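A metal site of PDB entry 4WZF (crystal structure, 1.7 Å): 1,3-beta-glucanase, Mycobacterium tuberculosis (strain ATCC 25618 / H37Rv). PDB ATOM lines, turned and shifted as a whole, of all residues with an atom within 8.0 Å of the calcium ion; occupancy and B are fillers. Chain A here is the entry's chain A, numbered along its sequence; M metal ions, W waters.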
ATOM      1  N   ASP A  60     -10.317  26.814  20.923  1.00  0.00           N
ATOM      2  CA  ASP A  60     -11.247  26.267  21.895  1.00  0.00           C
ATOM      3  C   ASP A  60     -11.271  24.760  21.724  1.00  0.00           C
ATOM      4  O   ASP A  60     -11.492  24.265  20.611  1.00  0.00           O
ATOM      5  CB  ASP A  60     -12.658  26.853  21.738  1.00  0.00           C
ATOM      6  CG  ASP A  60     -13.500  26.686  22.993  1.00  0.00           C
ATOM      7  OD1 ASP A  60     -13.152  25.829  23.825  1.00  0.00           O
ATOM      8  OD2 ASP A  60     -14.501  27.422  23.155  1.00  0.00           O
ATOM      9  N   GLU A  61     -10.995  24.035  22.799  1.00  0.00           N
ATOM     10  CA  GLU A  61     -11.103  22.584  22.785  1.00  0.00           C
ATOM     11  C   GLU A  61     -12.489  22.100  23.219  1.00  0.00           C
ATOM     12  O   GLU A  61     -12.771  20.892  23.178  1.00  0.00           O
ATOM     13  CB  GLU A  61     -10.030  21.981  23.702  1.00  0.00           C
ATOM     14  CG  GLU A  61      -8.631  22.446  23.383  1.00  0.00           C
ATOM     15  CD  GLU A  61      -8.193  22.100  21.963  1.00  0.00           C
ATOM     16  OE1 GLU A  61      -8.541  21.001  21.496  1.00  0.00           O
ATOM     17  OE2 GLU A  61      -7.498  22.917  21.323  1.00  0.00           O
ATOM     18  N   PHE A  62     -13.343  23.029  23.646  1.00  0.00           N
ATOM     19  CA  PHE A  62     -14.748  22.742  23.960  1.00  0.00           C
ATOM     20  C   PHE A  62     -14.914  21.737  25.090  1.00  0.00           C
ATOM     21  O   PHE A  62     -15.837  20.936  25.103  1.00  0.00           O
ATOM     22  CB  PHE A  62     -15.503  22.260  22.713  1.00  0.00           C
ATOM     23  CG  PHE A  62     -15.574  23.285  21.620  1.00  0.00           C
ATOM     24  CD1 PHE A  62     -16.154  24.522  21.866  1.00  0.00           C
ATOM     25  CD2 PHE A  62     -15.062  23.034  20.349  1.00  0.00           C
ATOM     26  CE1 PHE A  62     -16.218  25.494  20.864  1.00  0.00           C
ATOM     27  CE2 PHE A  62     -15.118  24.003  19.354  1.00  0.00           C
ATOM     28  CZ  PHE A  62     -15.696  25.233  19.611  1.00  0.00           C
ATOM     29  N   ASP A  63     -13.986  21.783  26.040  1.00  0.00           N
ATOM     30  CA  ASP A  63     -14.113  21.017  27.286  1.00  0.00           C
ATOM     31  C   ASP A  63     -15.170  21.652  28.170  1.00  0.00           C
ATOM     32  O   ASP A  63     -15.369  22.864  28.141  1.00  0.00           O
ATOM     33  CB  ASP A  63     -12.780  20.971  28.023  1.00  0.00           C
ATOM     34  CG  ASP A  63     -11.733  20.168  27.294  1.00  0.00           C
ATOM     35  OD1 ASP A  63     -12.084  19.107  26.741  1.00  0.00           O
ATOM     36  OD2 ASP A  63     -10.562  20.592  27.272  1.00  0.00           O
ATOM     37  N   GLY A  64     -15.834  20.833  28.977  1.00  0.00           N
ATOM     38  CA  GLY A  64     -16.844  21.366  29.878  1.00  0.00           C
ATOM     39  C   GLY A  64     -18.016  20.426  30.038  1.00  0.00           C
ATOM     40  O   GLY A  64     -18.181  19.494  29.263  1.00  0.00           O
ATOM     41  N   ASP A 109     -21.199  18.952  24.777  1.00  0.00           N
ATOM     42  CA  ASP A 109     -21.804  17.650  25.075  1.00  0.00           C
ATOM     43  C   ASP A 109     -21.209  16.932  26.291  1.00  0.00           C
ATOM     44  O   ASP A 109     -21.690  15.844  26.680  1.00  0.00           O
ATOM     45  CB  ASP A 109     -21.740  16.715  23.859  1.00  0.00           C
ATOM     46  CG  ASP A 109     -20.327  16.312  23.457  1.00  0.00           C
ATOM     47  OD1 ASP A 109     -19.327  16.809  24.037  1.00  0.00           O
ATOM     48  OD2 ASP A 109     -20.216  15.495  22.506  1.00  0.00           O
ATOM     49  N   ASN A 111     -18.321  15.717  26.356  1.00  0.00           N
ATOM     50  CA  ASN A 111     -17.283  14.866  25.795  1.00  0.00           C
ATOM     51  C   ASN A 111     -16.257  15.657  24.984  1.00  0.00           C
ATOM     52  O   ASN A 111     -15.621  15.111  24.087  1.00  0.00           O
ATOM     53  CB  ASN A 111     -17.904  13.797  24.909  1.00  0.00           C
ATOM     54  CG  ASN A 111     -18.882  12.925  25.673  1.00  0.00           C
ATOM     55  OD1 ASN A 111     -18.572  12.455  26.772  1.00  0.00           O
ATOM     56  ND2 ASN A 111     -20.067  12.720  25.119  1.00  0.00           N
ATOM     57  N   SER A 112     -16.153  16.955  25.275  1.00  0.00           N
ATOM     58  CA  SER A 112     -15.224  17.857  24.610  1.00  0.00           C
ATOM     59  C   SER A 112     -15.630  18.163  23.154  1.00  0.00           C
ATOM     60  O   SER A 112     -14.765  18.405  22.320  1.00  0.00           O
ATOM     61  CB  SER A 112     -13.800  17.304  24.657  1.00  0.00           C
ATOM     62  OG  SER A 112     -12.850  18.317  24.379  1.00  0.00           O
ATOM     63  N   ASN A 113     -16.922  18.145  22.861  1.00  0.00           N
ATOM     64  CA  ASN A 113     -17.443  18.671  21.586  1.00  0.00           C
ATOM     65  C   ASN A 113     -18.429  19.809  21.772  1.00  0.00           C
ATOM     66  O   ASN A 113     -19.241  19.810  22.704  1.00  0.00           O
ATOM     67  CB  ASN A 113     -18.148  17.590  20.759  1.00  0.00           C
ATOM     68  CG  ASN A 113     -17.277  16.383  20.493  1.00  0.00           C
ATOM     69  OD1 ASN A 113     -16.177  16.503  19.951  1.00  0.00           O
ATOM     70  ND2 ASN A 113     -17.765  15.201  20.887  1.00  0.00           N
ATOM     71  N   LEU A 114     -18.353  20.775  20.873  1.00  0.00           N
ATOM     72  CA  LEU A 114     -19.447  21.709  20.633  1.00  0.00           C
ATOM     73  C   LEU A 114     -20.505  20.986  19.828  1.00  0.00           C
ATOM     74  O   LEU A 114     -20.185  20.269  18.876  1.00  0.00           O
ATOM     75  CB  LEU A 114     -18.942  22.923  19.875  1.00  0.00           C
ATOM     76  CG  LEU A 114     -20.017  23.859  19.363  1.00  0.00           C
ATOM     77  CD1 LEU A 114     -20.688  24.563  20.549  1.00  0.00           C
ATOM     78  CD2 LEU A 114     -19.392  24.867  18.389  1.00  0.00           C
ATOM     79  N   ARG A 145     -11.879  20.576  13.671  1.00  0.00           N
ATOM     80  CA  ARG A 145     -12.182  19.146  13.566  1.00  0.00           C
ATOM     81  C   ARG A 145     -13.679  18.968  13.737  1.00  0.00           C
ATOM     82  O   ARG A 145     -14.243  19.308  14.782  1.00  0.00           O
ATOM     83  CB  ARG A 145     -11.404  18.351  14.618  1.00  0.00           C
ATOM     84  CG  ARG A 145     -11.645  16.843  14.553  1.00  0.00           C
ATOM     85  CD  ARG A 145     -10.535  16.082  15.267  1.00  0.00           C
ATOM     86  NE  ARG A 145     -10.683  14.635  15.098  1.00  0.00           N
ATOM     87  CZ  ARG A 145     -10.279  13.959  14.029  1.00  0.00           C
ATOM     88  NH1 ARG A 145      -9.716  14.609  13.009  1.00  0.00           N
ATOM     89  NH2 ARG A 145     -10.441  12.642  13.970  1.00  0.00           N
ATOM     90  N   TRP A 209     -15.244  11.973  11.061  1.00  0.00           N
ATOM     91  CA  TRP A 209     -14.462  13.082  11.598  1.00  0.00           C
ATOM     92  C   TRP A 209     -13.467  13.565  10.544  1.00  0.00           C
ATOM     93  O   TRP A 209     -12.754  12.767   9.929  1.00  0.00           O
ATOM     94  CB  TRP A 209     -13.736  12.643  12.872  1.00  0.00           C
ATOM     95  CG  TRP A 209     -14.597  12.614  14.087  1.00  0.00           C
ATOM     96  CD1 TRP A 209     -15.092  11.508  14.736  1.00  0.00           C
ATOM     97  CD2 TRP A 209     -15.083  13.750  14.811  1.00  0.00           C
ATOM     98  NE1 TRP A 209     -15.856  11.893  15.813  1.00  0.00           N
ATOM     99  CE2 TRP A 209     -15.866  13.262  15.886  1.00  0.00           C
ATOM    100  CE3 TRP A 209     -14.938  15.131  14.657  1.00  0.00           C
ATOM    101  CZ2 TRP A 209     -16.485  14.105  16.795  1.00  0.00           C
ATOM    102  CZ3 TRP A 209     -15.547  15.964  15.566  1.00  0.00           C
ATOM    103  CH2 TRP A 209     -16.311  15.456  16.624  1.00  0.00           C
ATOM    104  N   VAL A 288     -18.234  19.645  16.793  1.00  0.00           N
ATOM    105  CA  VAL A 288     -16.900  20.233  16.613  1.00  0.00           C
ATOM    106  C   VAL A 288     -16.011  19.900  17.810  1.00  0.00           C
ATOM    107  O   VAL A 288     -16.259  20.322  18.928  1.00  0.00           O
ATOM    108  CB  VAL A 288     -16.977  21.785  16.433  1.00  0.00           C
ATOM    109  CG1 VAL A 288     -15.634  22.326  15.959  1.00  0.00           C
ATOM    110  CG2 VAL A 288     -18.071  22.165  15.435  1.00  0.00           C
ATOM    111  N   ASP A 289     -14.951  19.153  17.543  1.00  0.00           N
ATOM    112  CA  ASP A 289     -14.044  18.740  18.613  1.00  0.00           C
ATOM    113  C   ASP A 289     -13.160  19.907  19.051  1.00  0.00           C
ATOM    114  O   ASP A 289     -12.902  20.096  20.250  1.00  0.00           O
ATOM    115  CB  ASP A 289     -13.228  17.543  18.128  1.00  0.00           C
ATOM    116  CG  ASP A 289     -12.318  16.959  19.208  1.00  0.00           C
ATOM    117  OD1 ASP A 289     -12.409  17.334  20.405  1.00  0.00           O
ATOM    118  OD2 ASP A 289     -11.499  16.093  18.822  1.00  0.00           O
ATOM    119  N   TRP A 290     -12.704  20.707  18.085  1.00  0.00           N
ATOM    120  CA  TRP A 290     -11.880  21.878  18.397  1.00  0.00           C
ATOM    121  C   TRP A 290     -11.797  22.834  17.221  1.00  0.00           C
ATOM    122  O   TRP A 290     -12.083  22.462  16.091  1.00  0.00           O
ATOM    123  CB  TRP A 290     -10.444  21.476  18.809  1.00  0.00           C
ATOM    124  CG  TRP A 290      -9.754  20.426  17.979  1.00  0.00           C
ATOM    125  CD1 TRP A 290      -9.620  19.101  18.297  1.00  0.00           C
ATOM    126  CD2 TRP A 290      -9.053  20.606  16.731  1.00  0.00           C
ATOM    127  NE1 TRP A 290      -8.916  18.446  17.330  1.00  0.00           N
ATOM    128  CE2 TRP A 290      -8.541  19.345  16.359  1.00  0.00           C
ATOM    129  CE3 TRP A 290      -8.798  21.711  15.906  1.00  0.00           C
ATOM    130  CZ2 TRP A 290      -7.820  19.135  15.184  1.00  0.00           C
ATOM    131  CZ3 TRP A 290      -8.071  21.506  14.726  1.00  0.00           C
ATOM    132  CH2 TRP A 290      -7.584  20.230  14.382  1.00  0.00           C
ATOM    133  N   VAL A 291     -11.419  24.079  17.532  1.00  0.00           N
ATOM    134  CA  VAL A 291     -11.026  25.083  16.543  1.00  0.00           C
ATOM    135  C   VAL A 291      -9.659  25.588  16.970  1.00  0.00           C
ATOM    136  O   VAL A 291      -9.517  25.989  18.118  1.00  0.00           O
ATOM    137  CB  VAL A 291     -12.002  26.292  16.481  1.00  0.00           C
ATOM    138  CG1 VAL A 291     -11.438  27.407  15.566  1.00  0.00           C
ATOM    139  CG2 VAL A 291     -13.380  25.864  16.032  1.00  0.00           C
ATOM    140  N   ARG A 292      -8.670  25.578  16.088  1.00  0.00           N
ATOM    141  CA  ARG A 292      -7.350  26.097  16.428  1.00  0.00           C
ATOM    142  C   ARG A 292      -6.856  27.071  15.357  1.00  0.00           C
ATOM    143  O   ARG A 292      -7.075  26.840  14.175  1.00  0.00           O
ATOM    144  CB  ARG A 292      -6.339  24.959  16.576  1.00  0.00           C
ATOM    145  CG  ARG A 292      -6.649  24.041  17.749  1.00  0.00           C
ATOM    146  CD  ARG A 292      -5.912  22.727  17.640  1.00  0.00           C
ATOM    147  NE  ARG A 292      -6.333  21.812  18.687  1.00  0.00           N
ATOM    148  CZ  ARG A 292      -6.062  20.513  18.704  1.00  0.00           C
ATOM    149  NH1 ARG A 292      -5.359  19.954  17.725  1.00  0.00           N
ATOM    150  NH2 ARG A 292      -6.507  19.761  19.711  1.00  0.00           N
HETATM  151 CA    CA M   1     -12.484  18.738  22.113  1.00  0.00          CA
HETATM  152  O   HOH W   1     -11.353  16.464  22.783  1.00  0.00           O
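The calcium ion is bound by OD1 of Asp 289 (2.2 Å), O of Ser 112 (2.3 Å), OG of Ser 112 (2.3 Å), O of Asp 289 (2.3 Å), O of Glu 61 (2.4 Å) and water W1 (2.6 Å).
The nearest printed residue that does not touch the calcium ion is Trp 290 (4.5 Å).
N of Asp 289 is in hydrogen-bond range of O of Arg 145, at 2.9 Å. OG of Ser 112 sits close to OD1 of Asp 63 (2.6 Å). The backbone NH of Ser 112 lies within hydrogen-bond range of the side-chain carboxylate of Asp 109 (3.4 Å). NH2 of Arg 292 lies within salt-bridge range of OE1 of Glu 61 (3.0 Å).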
